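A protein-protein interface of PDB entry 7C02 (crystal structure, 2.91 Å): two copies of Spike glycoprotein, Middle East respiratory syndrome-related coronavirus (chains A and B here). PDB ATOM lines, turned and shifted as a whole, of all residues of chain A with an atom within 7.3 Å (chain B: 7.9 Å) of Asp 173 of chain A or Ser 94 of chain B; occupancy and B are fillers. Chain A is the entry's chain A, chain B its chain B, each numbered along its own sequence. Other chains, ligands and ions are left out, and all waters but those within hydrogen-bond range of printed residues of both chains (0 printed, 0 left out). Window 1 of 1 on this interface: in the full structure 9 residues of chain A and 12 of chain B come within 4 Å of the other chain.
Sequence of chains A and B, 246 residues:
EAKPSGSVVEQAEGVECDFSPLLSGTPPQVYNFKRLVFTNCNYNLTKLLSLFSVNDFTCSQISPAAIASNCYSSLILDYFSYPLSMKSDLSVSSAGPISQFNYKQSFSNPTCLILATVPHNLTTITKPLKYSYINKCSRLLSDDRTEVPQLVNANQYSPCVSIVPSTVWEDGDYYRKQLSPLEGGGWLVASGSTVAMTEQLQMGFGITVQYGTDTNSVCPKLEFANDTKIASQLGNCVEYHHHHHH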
ATOM      1  N   ASN A 135     -12.689 -11.214 -30.969  1.00  0.00           N
ATOM      2  CA  ASN A 135     -13.143 -10.757 -32.276  1.00  0.00           C
ATOM      3  C   ASN A 135     -12.311  -9.609 -32.836  1.00  0.00           C
ATOM      4  O   ASN A 135     -12.435  -9.303 -34.028  1.00  0.00           O
ATOM      5  CB  ASN A 135     -14.618 -10.330 -32.207  1.00  0.00           C
ATOM      6  CG  ASN A 135     -14.824  -9.061 -31.400  1.00  0.00           C
ATOM      7  OD1 ASN A 135     -14.544  -7.956 -31.869  1.00  0.00           O
ATOM      8  ND2 ASN A 135     -15.329  -9.213 -30.184  1.00  0.00           N
ATOM      9  N   ILE A 163      -5.027  -8.838 -21.441  1.00  0.00           N
ATOM     10  CA  ILE A 163      -6.151  -8.008 -21.030  1.00  0.00           C
ATOM     11  C   ILE A 163      -7.495  -8.680 -21.268  1.00  0.00           C
ATOM     12  O   ILE A 163      -8.528  -8.108 -20.909  1.00  0.00           O
ATOM     13  CB  ILE A 163      -6.117  -6.635 -21.730  1.00  0.00           C
ATOM     14  CG1 ILE A 163      -6.376  -6.798 -23.230  1.00  0.00           C
ATOM     15  CG2 ILE A 163      -4.789  -5.944 -21.484  1.00  0.00           C
ATOM     16  CD1 ILE A 163      -6.386  -5.493 -23.995  1.00  0.00           C
ATOM     17  N   VAL A 164      -7.517  -9.868 -21.853  1.00  0.00           N
ATOM     18  CA  VAL A 164      -8.748 -10.612 -22.118  1.00  0.00           C
ATOM     19  C   VAL A 164      -8.818 -11.775 -21.138  1.00  0.00           C
ATOM     20  O   VAL A 164      -7.877 -12.574 -21.076  1.00  0.00           O
ATOM     21  CB  VAL A 164      -8.809 -11.123 -23.570  1.00  0.00           C
ATOM     22  CG1 VAL A 164     -10.004 -12.045 -23.760  1.00  0.00           C
ATOM     23  CG2 VAL A 164      -8.872  -9.955 -24.542  1.00  0.00           C
ATOM     24  N   PRO A 165      -9.894 -11.910 -20.368  1.00  0.00           N
ATOM     25  CA  PRO A 165      -9.980 -13.004 -19.397  1.00  0.00           C
ATOM     26  C   PRO A 165     -10.164 -14.351 -20.080  1.00  0.00           C
ATOM     27  O   PRO A 165     -10.498 -14.445 -21.263  1.00  0.00           O
ATOM     28  CB  PRO A 165     -11.206 -12.638 -18.557  1.00  0.00           C
ATOM     29  CG  PRO A 165     -12.060 -11.846 -19.488  1.00  0.00           C
ATOM     30  CD  PRO A 165     -11.113 -11.081 -20.375  1.00  0.00           C
ATOM     31  N   THR A 167     -12.510 -16.195 -19.840  1.00  0.00           N
ATOM     32  CA  THR A 167     -13.902 -16.350 -20.249  1.00  0.00           C
ATOM     33  C   THR A 167     -14.493 -14.962 -20.437  1.00  0.00           C
ATOM     34  O   THR A 167     -14.474 -14.153 -19.504  1.00  0.00           O
ATOM     35  CB  THR A 167     -14.706 -17.139 -19.212  1.00  0.00           C
ATOM     36  OG1 THR A 167     -13.944 -18.267 -18.763  1.00  0.00           O
ATOM     37  CG2 THR A 167     -16.018 -17.626 -19.810  1.00  0.00           C
ATOM     38  N   VAL A 168     -15.010 -14.685 -21.631  1.00  0.00           N
ATOM     39  CA  VAL A 168     -15.648 -13.398 -21.884  1.00  0.00           C
ATOM     40  C   VAL A 168     -16.946 -13.331 -21.089  1.00  0.00           C
ATOM     41  O   VAL A 168     -17.826 -14.188 -21.234  1.00  0.00           O
ATOM     42  CB  VAL A 168     -15.895 -13.184 -23.382  1.00  0.00           C
ATOM     43  CG1 VAL A 168     -16.703 -11.915 -23.603  1.00  0.00           C
ATOM     44  CG2 VAL A 168     -14.574 -13.107 -24.129  1.00  0.00           C
ATOM     45  N   TRP A 169     -17.067 -12.309 -20.240  1.00  0.00           N
ATOM     46  CA  TRP A 169     -18.247 -12.177 -19.392  1.00  0.00           C
ATOM     47  C   TRP A 169     -19.492 -11.888 -20.221  1.00  0.00           C
ATOM     48  O   TRP A 169     -20.494 -12.607 -20.129  1.00  0.00           O
ATOM     49  CB  TRP A 169     -18.023 -11.079 -18.353  1.00  0.00           C
ATOM     50  CG  TRP A 169     -19.168 -10.911 -17.407  1.00  0.00           C
ATOM     51  CD1 TRP A 169     -20.108  -9.923 -17.423  1.00  0.00           C
ATOM     52  CD2 TRP A 169     -19.497 -11.759 -16.300  1.00  0.00           C
ATOM     53  NE1 TRP A 169     -21.002 -10.102 -16.395  1.00  0.00           N
ATOM     54  CE2 TRP A 169     -20.649 -11.222 -15.692  1.00  0.00           C
ATOM     55  CE3 TRP A 169     -18.930 -12.920 -15.765  1.00  0.00           C
ATOM     56  CZ2 TRP A 169     -21.243 -11.806 -14.575  1.00  0.00           C
ATOM     57  CZ3 TRP A 169     -19.521 -13.498 -14.657  1.00  0.00           C
ATOM     58  CH2 TRP A 169     -20.666 -12.940 -14.074  1.00  0.00           C
ATOM     59  N   GLU A 170     -19.447 -10.837 -21.036  1.00  0.00           N
ATOM     60  CA  GLU A 170     -20.588 -10.400 -21.825  1.00  0.00           C
ATOM     61  C   GLU A 170     -20.152 -10.192 -23.266  1.00  0.00           C
ATOM     62  O   GLU A 170     -19.097  -9.604 -23.525  1.00  0.00           O
ATOM     63  CB  GLU A 170     -21.183  -9.102 -21.264  1.00  0.00           C
ATOM     64  CG  GLU A 170     -22.672  -8.934 -21.505  1.00  0.00           C
ATOM     65  CD  GLU A 170     -23.285  -7.868 -20.619  1.00  0.00           C
ATOM     66  OE1 GLU A 170     -22.527  -7.189 -19.895  1.00  0.00           O
ATOM     67  OE2 GLU A 170     -24.522  -7.705 -20.647  1.00  0.00           O
ATOM     68  N   ASP A 171     -20.962 -10.687 -24.200  1.00  0.00           N
ATOM     69  CA  ASP A 171     -20.660 -10.526 -25.617  1.00  0.00           C
ATOM     70  C   ASP A 171     -20.616  -9.046 -25.975  1.00  0.00           C
ATOM     71  O   ASP A 171     -21.590  -8.317 -25.763  1.00  0.00           O
ATOM     72  CB  ASP A 171     -21.706 -11.252 -26.462  1.00  0.00           C
ATOM     73  CG  ASP A 171     -21.415 -11.170 -27.948  1.00  0.00           C
ATOM     74  OD1 ASP A 171     -20.769 -12.097 -28.479  1.00  0.00           O
ATOM     75  OD2 ASP A 171     -21.834 -10.182 -28.586  1.00  0.00           O
ATOM     76  N   GLY A 172     -19.485  -8.606 -26.518  1.00  0.00           N
ATOM     77  CA  GLY A 172     -19.279  -7.212 -26.845  1.00  0.00           C
ATOM     78  C   GLY A 172     -18.405  -6.451 -25.873  1.00  0.00           C
ATOM     79  O   GLY A 172     -18.175  -5.254 -26.086  1.00  0.00           O
ATOM     80  N   ASP A 173     -17.922  -7.099 -24.814  1.00  0.00           N
ATOM     81  CA  ASP A 173     -17.029  -6.443 -23.870  1.00  0.00           C
ATOM     82  C   ASP A 173     -15.774  -5.947 -24.578  1.00  0.00           C
ATOM     83  O   ASP A 173     -15.292  -6.558 -25.536  1.00  0.00           O
ATOM     84  CB  ASP A 173     -16.650  -7.402 -22.739  1.00  0.00           C
ATOM     85  CG  ASP A 173     -17.683  -7.435 -21.630  1.00  0.00           C
ATOM     86  OD1 ASP A 173     -18.386  -6.421 -21.438  1.00  0.00           O
ATOM     87  OD2 ASP A 173     -17.793  -8.477 -20.949  1.00  0.00           O
ATOM     88  N   TYR A 174     -15.242  -4.829 -24.095  1.00  0.00           N
ATOM     89  CA  TYR A 174     -14.077  -4.193 -24.692  1.00  0.00           C
ATOM     90  C   TYR A 174     -12.963  -4.107 -23.660  1.00  0.00           C
ATOM     91  O   TYR A 174     -13.217  -3.862 -22.477  1.00  0.00           O
ATOM     92  CB  TYR A 174     -14.419  -2.789 -25.206  1.00  0.00           C
ATOM     93  CG  TYR A 174     -14.469  -2.664 -26.712  1.00  0.00           C
ATOM     94  CD1 TYR A 174     -15.532  -3.188 -27.438  1.00  0.00           C
ATOM     95  CD2 TYR A 174     -13.458  -2.014 -27.408  1.00  0.00           C
ATOM     96  CE1 TYR A 174     -15.583  -3.071 -28.815  1.00  0.00           C
ATOM     97  CE2 TYR A 174     -13.501  -1.893 -28.784  1.00  0.00           C
ATOM     98  CZ  TYR A 174     -14.564  -2.423 -29.482  1.00  0.00           C
ATOM     99  OH  TYR A 174     -14.610  -2.305 -30.853  1.00  0.00           O
ATOM    100  N   TYR A 175     -11.727  -4.298 -24.117  1.00  0.00           N
ATOM    101  CA  TYR A 175     -10.562  -4.278 -23.245  1.00  0.00           C
ATOM    102  C   TYR A 175      -9.500  -3.375 -23.848  1.00  0.00           C
ATOM    103  O   TYR A 175      -9.272  -3.396 -25.062  1.00  0.00           O
ATOM    104  CB  TYR A 175      -9.995  -5.694 -23.048  1.00  0.00           C
ATOM    105  CG  TYR A 175     -11.054  -6.760 -22.871  1.00  0.00           C
ATOM    106  CD1 TYR A 175     -11.468  -7.148 -21.606  1.00  0.00           C
ATOM    107  CD2 TYR A 175     -11.638  -7.382 -23.969  1.00  0.00           C
ATOM    108  CE1 TYR A 175     -12.435  -8.120 -21.437  1.00  0.00           C
ATOM    109  CE2 TYR A 175     -12.608  -8.355 -23.809  1.00  0.00           C
ATOM    110  CZ  TYR A 175     -13.001  -8.720 -22.539  1.00  0.00           C
ATOM    111  OH  TYR A 175     -13.964  -9.689 -22.367  1.00  0.00           O
ATOM    112  N   ARG A 176      -8.846  -2.585 -22.998  1.00  0.00           N
ATOM    113  CA  ARG A 176      -7.795  -1.680 -23.441  1.00  0.00           C
ATOM    114  C   ARG A 176      -6.692  -1.619 -22.395  1.00  0.00           C
ATOM    115  O   ARG A 176      -6.935  -1.805 -21.199  1.00  0.00           O
ATOM    116  CB  ARG A 176      -8.335  -0.271 -23.728  1.00  0.00           C
ATOM    117  CG  ARG A 176      -9.419  -0.222 -24.800  1.00  0.00           C
ATOM    118  CD  ARG A 176      -9.663   1.187 -25.312  1.00  0.00           C
ATOM    119  NE  ARG A 176     -11.060   1.583 -25.145  1.00  0.00           N
ATOM    120  CZ  ARG A 176     -11.844   1.992 -26.136  1.00  0.00           C
ATOM    121  NH1 ARG A 176     -11.369   2.062 -27.372  1.00  0.00           N
ATOM    122  NH2 ARG A 176     -13.102   2.332 -25.892  1.00  0.00           N
ATOM    123  N   ALA A 190      -8.885  -4.509 -27.444  1.00  0.00           N
ATOM    124  CA  ALA A 190      -9.448  -5.804 -27.789  1.00  0.00           C
ATOM    125  C   ALA A 190     -10.926  -5.838 -27.428  1.00  0.00           C
ATOM    126  O   ALA A 190     -11.383  -5.106 -26.547  1.00  0.00           O
ATOM    127  CB  ALA A 190      -8.710  -6.948 -27.081  1.00  0.00           C
ATOM    128  N   SER A 191     -11.670  -6.699 -28.124  1.00  0.00           N
ATOM    129  CA  SER A 191     -13.049  -7.009 -27.773  1.00  0.00           C
ATOM    130  C   SER A 191     -13.264  -8.510 -27.897  1.00  0.00           C
ATOM    131  O   SER A 191     -12.692  -9.154 -28.782  1.00  0.00           O
ATOM    132  CB  SER A 191     -14.046  -6.261 -28.668  1.00  0.00           C
ATOM    133  OG  SER A 191     -15.352  -6.797 -28.532  1.00  0.00           O
ATOM    134  N   GLY A 192     -14.091  -9.061 -27.016  1.00  0.00           N
ATOM    135  CA  GLY A 192     -14.391 -10.481 -27.020  1.00  0.00           C
ATOM    136  C   GLY A 192     -15.850 -10.748 -27.340  1.00  0.00           C
ATOM    137  O   GLY A 192     -16.721  -9.917 -27.080  1.00  0.00           O
ATOM    138  N   SER A 193     -16.112 -11.925 -27.906  1.00  0.00           N
ATOM    139  CA  SER A 193     -17.468 -12.379 -28.167  1.00  0.00           C
ATOM    140  C   SER A 193     -17.652 -13.781 -27.603  1.00  0.00           C
ATOM    141  O   SER A 193     -16.684 -14.488 -27.316  1.00  0.00           O
ATOM    142  CB  SER A 193     -17.789 -12.363 -29.672  1.00  0.00           C
ATOM    143  OG  SER A 193     -17.183 -11.252 -30.311  1.00  0.00           O
ATOM    144  N   THR A 194     -18.916 -14.180 -27.451  1.00  0.00           N
ATOM    145  CA  THR A 194     -19.284 -15.464 -26.865  1.00  0.00           C
ATOM    146  C   THR A 194     -20.297 -16.174 -27.752  1.00  0.00           C
ATOM    147  O   THR A 194     -21.086 -15.541 -28.459  1.00  0.00           O
ATOM    148  CB  THR A 194     -19.873 -15.333 -25.436  1.00  0.00           C
ATOM    149  OG1 THR A 194     -21.286 -15.129 -25.503  1.00  0.00           O
ATOM    150  CG2 THR A 194     -19.233 -14.190 -24.678  1.00  0.00           C
ATOM    151  N   ASP B  89      -8.845   4.621 -15.867  1.00  0.00           N
ATOM    152  CA  ASP B  89      -9.580   3.464 -15.359  1.00  0.00           C
ATOM    153  C   ASP B  89     -10.937   3.290 -16.030  1.00  0.00           C
ATOM    154  O   ASP B  89     -11.647   2.321 -15.734  1.00  0.00           O
ATOM    155  CB  ASP B  89      -9.753   3.584 -13.844  1.00  0.00           C
ATOM    156  CG  ASP B  89      -8.434   3.493 -13.103  1.00  0.00           C
ATOM    157  OD1 ASP B  89      -8.019   2.366 -12.762  1.00  0.00           O
ATOM    158  OD2 ASP B  89      -7.809   4.548 -12.867  1.00  0.00           O
ATOM    159  N   LEU B  90     -11.296   4.211 -16.922  1.00  0.00           N
ATOM    160  CA  LEU B  90     -12.504   4.177 -17.735  1.00  0.00           C
ATOM    161  C   LEU B  90     -12.232   3.701 -19.153  1.00  0.00           C
ATOM    162  O   LEU B  90     -13.081   3.025 -19.742  1.00  0.00           O
ATOM    163  CB  LEU B  90     -13.168   5.559 -17.782  1.00  0.00           C
ATOM    164  CG  LEU B  90     -13.952   5.960 -16.533  1.00  0.00           C
ATOM    165  CD1 LEU B  90     -14.586   7.335 -16.706  1.00  0.00           C
ATOM    166  CD2 LEU B  90     -15.004   4.915 -16.207  1.00  0.00           C
ATOM    167  N   SER B  91     -11.070   4.034 -19.703  1.00  0.00           N
ATOM    168  CA  SER B  91     -10.713   3.791 -21.092  1.00  0.00           C
ATOM    169  C   SER B  91     -10.171   2.382 -21.302  1.00  0.00           C
ATOM    170  O   SER B  91      -9.715   2.065 -22.404  1.00  0.00           O
ATOM    171  CB  SER B  91      -9.667   4.816 -21.543  1.00  0.00           C
ATOM    172  OG  SER B  91      -9.899   6.080 -20.945  1.00  0.00           O
ATOM    173  N   VAL B  92     -10.168   1.566 -20.249  1.00  0.00           N
ATOM    174  CA  VAL B  92      -9.586   0.228 -20.220  1.00  0.00           C
ATOM    175  C   VAL B  92     -10.650  -0.868 -20.272  1.00  0.00           C
ATOM    176  O   VAL B  92     -10.321  -2.047 -20.112  1.00  0.00           O
ATOM    177  CB  VAL B  92      -8.702   0.040 -18.981  1.00  0.00           C
ATOM    178  CG1 VAL B  92      -7.445   0.880 -19.088  1.00  0.00           C
ATOM    179  CG2 VAL B  92      -9.484   0.392 -17.729  1.00  0.00           C
ATOM    180  N   SER B  93     -11.910  -0.517 -20.543  1.00  0.00           N
ATOM    181  CA  SER B  93     -13.015  -0.745 -19.622  1.00  0.00           C
ATOM    182  C   SER B  93     -13.035  -2.122 -18.961  1.00  0.00           C
ATOM    183  O   SER B  93     -12.981  -2.211 -17.728  1.00  0.00           O
ATOM    184  CB  SER B  93     -14.330  -0.524 -20.377  1.00  0.00           C
ATOM    185  OG  SER B  93     -14.228   0.541 -21.311  1.00  0.00           O
ATOM    186  N   SER B  94     -13.100  -3.212 -19.720  1.00  0.00           N
ATOM    187  CA  SER B  94     -13.240  -4.489 -19.024  1.00  0.00           C
ATOM    188  C   SER B  94     -11.910  -5.054 -18.530  1.00  0.00           C
ATOM    189  O   SER B  94     -11.901  -6.128 -17.918  1.00  0.00           O
ATOM    190  CB  SER B  94     -13.949  -5.514 -19.909  1.00  0.00           C
ATOM    191  OG  SER B  94     -15.348  -5.506 -19.674  1.00  0.00           O
ATOM    192  N   ALA B  95     -10.801  -4.347 -18.754  1.00  0.00           N
ATOM    193  CA  ALA B  95      -9.530  -4.695 -18.131  1.00  0.00           C
ATOM    194  C   ALA B  95      -9.414  -4.088 -16.739  1.00  0.00           C
ATOM    195  O   ALA B  95      -8.747  -4.657 -15.866  1.00  0.00           O
ATOM    196  CB  ALA B  95      -8.363  -4.241 -19.010  1.00  0.00           C
ATOM    197  N   GLY B  96     -10.039  -2.934 -16.529  1.00  0.00           N
ATOM    198  CA  GLY B  96     -10.042  -2.254 -15.257  1.00  0.00           C
ATOM    199  C   GLY B  96     -11.270  -2.597 -14.438  1.00  0.00           C
ATOM    200  O   GLY B  96     -12.225  -3.208 -14.927  1.00  0.00           O
ATOM    201  N   PRO B  97     -11.268  -2.199 -13.162  1.00  0.00           N
ATOM    202  CA  PRO B  97     -12.304  -2.663 -12.227  1.00  0.00           C
ATOM    203  C   PRO B  97     -13.584  -1.845 -12.269  1.00  0.00           C
ATOM    204  O   PRO B  97     -14.594  -2.283 -11.702  1.00  0.00           O
ATOM    205  CB  PRO B  97     -11.621  -2.542 -10.852  1.00  0.00           C
ATOM    206  CG  PRO B  97     -10.261  -1.911 -11.103  1.00  0.00           C
ATOM    207  CD  PRO B  97     -10.259  -1.367 -12.493  1.00  0.00           C
ATOM    208  N   ILE B  98     -13.571  -0.681 -12.920  1.00  0.00           N
ATOM    209  CA  ILE B  98     -14.759   0.166 -12.966  1.00  0.00           C
ATOM    210  C   ILE B  98     -15.846  -0.492 -13.806  1.00  0.00           C
ATOM    211  O   ILE B  98     -17.019  -0.516 -13.412  1.00  0.00           O
ATOM    212  CB  ILE B  98     -14.402   1.568 -13.494  1.00  0.00           C
ATOM    213  CG1 ILE B  98     -13.451   2.272 -12.525  1.00  0.00           C
ATOM    214  CG2 ILE B  98     -15.662   2.394 -13.688  1.00  0.00           C
ATOM    215  CD1 ILE B  98     -14.040   2.499 -11.152  1.00  0.00           C
ATOM    216  N   SER B  99     -15.490  -1.039 -14.964  1.00  0.00           N
ATOM    217  CA  SER B  99     -16.488  -1.684 -15.805  1.00  0.00           C
ATOM    218  C   SER B  99     -16.636  -3.167 -15.498  1.00  0.00           C
ATOM    219  O   SER B  99     -17.578  -3.796 -15.993  1.00  0.00           O
ATOM    220  CB  SER B  99     -16.128  -1.513 -17.285  1.00  0.00           C
ATOM    221  OG  SER B  99     -16.218  -0.158 -17.690  1.00  0.00           O
ATOM    222  N   GLN B 100     -15.728  -3.742 -14.704  1.00  0.00           N
ATOM    223  CA  GLN B 100     -15.956  -5.080 -14.169  1.00  0.00           C
ATOM    224  C   GLN B 100     -16.941  -5.060 -13.006  1.00  0.00           C
ATOM    225  O   GLN B 100     -17.873  -5.869 -12.959  1.00  0.00           O
ATOM    226  CB  GLN B 100     -14.633  -5.699 -13.715  1.00  0.00           C
ATOM    227  CG  GLN B 100     -13.890  -6.466 -14.786  1.00  0.00           C
ATOM    228  CD  GLN B 100     -12.390  -6.381 -14.606  1.00  0.00           C
ATOM    229  OE1 GLN B 100     -11.898  -5.737 -13.677  1.00  0.00           O
ATOM    230  NE2 GLN B 100     -11.652  -7.034 -15.492  1.00  0.00           N
ATOM    231  N   PHE B 101     -16.746  -4.139 -12.057  1.00  0.00           N
ATOM    232  CA  PHE B 101     -17.402  -4.220 -10.762  1.00  0.00           C
ATOM    233  C   PHE B 101     -18.283  -3.035 -10.390  1.00  0.00           C
ATOM    234  O   PHE B 101     -19.096  -3.177  -9.474  1.00  0.00           O
ATOM    235  CB  PHE B 101     -16.363  -4.411  -9.647  1.00  0.00           C
ATOM    236  CG  PHE B 101     -15.460  -5.589  -9.861  1.00  0.00           C
ATOM    237  CD1 PHE B 101     -15.983  -6.866  -9.988  1.00  0.00           C
ATOM    238  CD2 PHE B 101     -14.088  -5.421  -9.936  1.00  0.00           C
ATOM    239  CE1 PHE B 101     -15.154  -7.952 -10.186  1.00  0.00           C
ATOM    240  CE2 PHE B 101     -13.254  -6.503 -10.134  1.00  0.00           C
ATOM    241  CZ  PHE B 101     -13.787  -7.770 -10.259  1.00  0.00           C
ATOM    242  N   LYS B 104     -21.329  -0.032 -15.860  1.00  0.00           N
ATOM    243  CA  LYS B 104     -21.208  -0.388 -17.271  1.00  0.00           C
ATOM    244  C   LYS B 104     -22.487   0.022 -17.983  1.00  0.00           C
ATOM    245  O   LYS B 104     -23.580  -0.384 -17.579  1.00  0.00           O
ATOM    246  CB  LYS B 104     -20.951  -1.887 -17.441  1.00  0.00           C
ATOM    247  CG  LYS B 104     -20.338  -2.265 -18.781  1.00  0.00           C
ATOM    248  CD  LYS B 104     -19.620  -3.603 -18.697  1.00  0.00           C
ATOM    249  CE  LYS B 104     -20.430  -4.705 -19.360  1.00  0.00           C
ATOM    250  NZ  LYS B 104     -20.045  -6.055 -18.863  1.00  0.00           N
ATOM    251  N   GLN B 105     -22.349   0.822 -19.037  1.00  0.00           N
ATOM    252  CA  GLN B 105     -23.493   1.334 -19.773  1.00  0.00           C
ATOM    253  C   GLN B 105     -23.953   0.330 -20.830  1.00  0.00           C
ATOM    254  O   GLN B 105     -23.299  -0.682 -21.093  1.00  0.00           O
ATOM    255  CB  GLN B 105     -23.156   2.679 -20.414  1.00  0.00           C
ATOM    256  CG  GLN B 105     -23.117   3.831 -19.422  1.00  0.00           C
ATOM    257  CD  GLN B 105     -22.578   5.112 -20.026  1.00  0.00           C
ATOM    258  OE1 GLN B 105     -21.369   5.269 -20.200  1.00  0.00           O
ATOM    259  NE2 GLN B 105     -23.473   6.040 -20.344  1.00  0.00           N
ATOM    260  N   PHE B 107     -24.865  -1.796 -24.078  1.00  0.00           N
ATOM    261  CA  PHE B 107     -24.352  -2.117 -25.403  1.00  0.00           C
ATOM    262  C   PHE B 107     -25.383  -1.869 -26.493  1.00  0.00           C
ATOM    263  O   PHE B 107     -25.014  -1.559 -27.633  1.00  0.00           O
ATOM    264  CB  PHE B 107     -23.904  -3.581 -25.470  1.00  0.00           C
ATOM    265  CG  PHE B 107     -22.723  -3.902 -24.599  1.00  0.00           C
ATOM    266  CD1 PHE B 107     -21.932  -2.896 -24.068  1.00  0.00           C
ATOM    267  CD2 PHE B 107     -22.403  -5.219 -24.317  1.00  0.00           C
ATOM    268  CE1 PHE B 107     -20.848  -3.200 -23.267  1.00  0.00           C
ATOM    269  CE2 PHE B 107     -21.320  -5.529 -23.519  1.00  0.00           C
ATOM    270  CZ  PHE B 107     -20.541  -4.518 -22.993  1.00  0.00           C
ATOM    271  N   LEU B 151     -19.142 -10.137 -12.175  1.00  0.00           N
ATOM    272  CA  LEU B 151     -19.024  -8.907 -12.943  1.00  0.00           C
ATOM    273  C   LEU B 151     -20.386  -8.251 -13.165  1.00  0.00           C
ATOM    274  O   LEU B 151     -21.442  -8.868 -12.998  1.00  0.00           O
ATOM    275  CB  LEU B 151     -18.341  -9.176 -14.283  1.00  0.00           C
ATOM    276  CG  LEU B 151     -16.830  -8.927 -14.315  1.00  0.00           C
ATOM    277  CD1 LEU B 151     -16.109  -9.812 -13.313  1.00  0.00           C
ATOM    278  CD2 LEU B 151     -16.276  -9.141 -15.714  1.00  0.00           C
ATOM    279  N   VAL B 152     -20.344  -6.972 -13.543  1.00  0.00           N
ATOM    280  CA  VAL B 152     -21.539  -6.158 -13.737  1.00  0.00           C
ATOM    281  C   VAL B 152     -22.060  -6.333 -15.156  1.00  0.00           C
ATOM    282  O   VAL B 152     -21.298  -6.534 -16.109  1.00  0.00           O
ATOM    283  CB  VAL B 152     -21.232  -4.677 -13.433  1.00  0.00           C
ATOM    284  CG1 VAL B 152     -22.465  -3.807 -13.609  1.00  0.00           C
ATOM    285  CG2 VAL B 152     -20.711  -4.543 -12.035  1.00  0.00           C
ATOM    286  N   ASN B 153     -23.379  -6.260 -15.295  1.00  0.00           N
ATOM    287  CA  ASN B 153     -24.040  -6.225 -16.589  1.00  0.00           C
ATOM    288  C   ASN B 153     -24.445  -4.796 -16.935  1.00  0.00           C
ATOM    289  O   ASN B 153     -24.463  -3.904 -16.084  1.00  0.00           O
ATOM    290  CB  ASN B 153     -25.266  -7.140 -16.595  1.00  0.00           C
ATOM    291  CG  ASN B 153     -24.928  -8.568 -16.218  1.00  0.00           C
ATOM    292  OD1 ASN B 153     -23.824  -9.047 -16.477  1.00  0.00           O
ATOM    293  ND2 ASN B 153     -25.881  -9.260 -15.604  1.00  0.00           N
ATOM    294  N   ALA B 154     -24.770  -4.590 -18.208  1.00  0.00           N
ATOM    295  CA  ALA B 154     -25.205  -3.278 -18.667  1.00  0.00           C
ATOM    296  C   ALA B 154     -26.527  -2.891 -18.016  1.00  0.00           C
ATOM    297  O   ALA B 154     -27.456  -3.700 -17.932  1.00  0.00           O
ATOM    298  CB  ALA B 154     -25.341  -3.267 -20.189  1.00  0.00           C
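The side-chain amide oxygen of Asn 153 of chain B sits at hydrogen-bond distance from the indole nitrogen of Trp 169 of chain A (3.0 Å).
The side-chain carboxylate (OE1) of Glu 170 of chain A lies within salt-bridge range of the side-chain amino group (NZ) of Lys 104 of chain B, 2.9 Å away.
The side-chain carboxylate of Asp 173 of chain A lies within salt-bridge range of the side-chain amino group of Lys 104 of chain B, at 3.1 Å.
The backbone carbonyl oxygen of Tyr 174 of chain A lies within hydrogen-bond range of the backbone NH of Ser 94 of chain B, 2.8 Å away.
The backbone carbonyl oxygen (O) of Ser 91 of chain B sits close to the guanidinium group (NE) of Arg 176 of chain A (3.1 Å).
The backbone NH (N) of Arg 176 of chain A sits at hydrogen-bond distance from the backbone carbonyl oxygen (O) of Val 92 of chain B (3.3 Å).
N of Thr 194 of chain A sits at hydrogen-bond distance from OD1 of Asp 171 of chain A, at 3.0 Å.
The backbone carbonyl oxygen (O) of Asp 173 of chain A sits at hydrogen-bond distance from the side-chain hydroxyl (OG) of Ser 191 of chain A (3.0 Å).
The backbone carbonyl oxygen (O) of Gln 100 of chain B sits at hydrogen-bond distance from the backbone NH (N) of Val 152 of chain B (2.8 Å).
O of Val 152 of chain B sits at hydrogen-bond distance from NZ of Lys 104 of chain B.
Leu 151 of chain B touches Trp 169 of chain A (O to CZ2, 3.3 Å).
O of Val 152 of chain B touches NE1 of Trp 169 of chain A, at 3.6 Å.
Glu 170 of chain A touches Asn 153 of chain B (OE1 to CA, 3.8 Å).
Asp 171 of chain A touches Phe 107 of chain B.
Phe 107 of chain B touches Gly 172 of chain A.
Ser 94 of chain B touches Asp 173 of chain A (OG to CG, 3.6 Å).
OD1 of Asp 173 of chain A touches CZ of Phe 107 of chain B, 3.3 Å away.
CA of Tyr 175 of chain A touches O of Val 92 of chain B (3.9 Å).
CB of Ala 95 of chain B touches O of Arg 176 of chain A, 3.6 Å away.
Printed residues of chain B within 4 Å of Asp 173 of chain A: Ser 94, Lys 104 and Phe 107.
Of chain A, only Asp 173 (3.6 Å), Tyr 174 (2.8 Å) and Tyr 175 (3.4 Å) come within 4 Å of Ser 94 of chain B.
Of chain B, only Phe 107 comes within 4 Å of Gly 172 of chain A.
Of the printed residues of chain A, Lys 104 of chain B touches Glu 170 and Asp 173.
Of the printed residues of chain B, Trp 169 of chain A touches Leu 151, Val 152 and Asn 153.
Gly 192 of chain A touches none of the printed residues of chain B.
The nearest residue of chain B that does not touch Asp 173 of chain A is Leu 151 of chain B (5.5 Å).
The nearest residue of chain A that does not touch Ser 94 of chain B is Ile 163 of chain A (4.9 Å).
Of the 20 printed residues of chain B, 11 touch a printed residue of chain A.
Hydrophobic or aromatic side chains of chain B that line the printed part of chain A: Val 92, Ala 95, Phe 107 and Leu 151.
Along chain A the printed residues that touch a printed residue of chain B span positions 169 to 176.
Among the printed residues, 18 pairs touch across the chains.
Among the printed residues, Asp or Glu carboxylates within 4 Å of a Lys or Arg side-chain nitrogen of the other chain: Glu 170 of chain A with Lys 104 of chain B and Asp 173 of chain A with Lys 104 of chain B.
No position is printed for both chains.
Of the 18 pairs that touch across the chains among the printed residues, none has its exchanged pair printed and touching as well.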
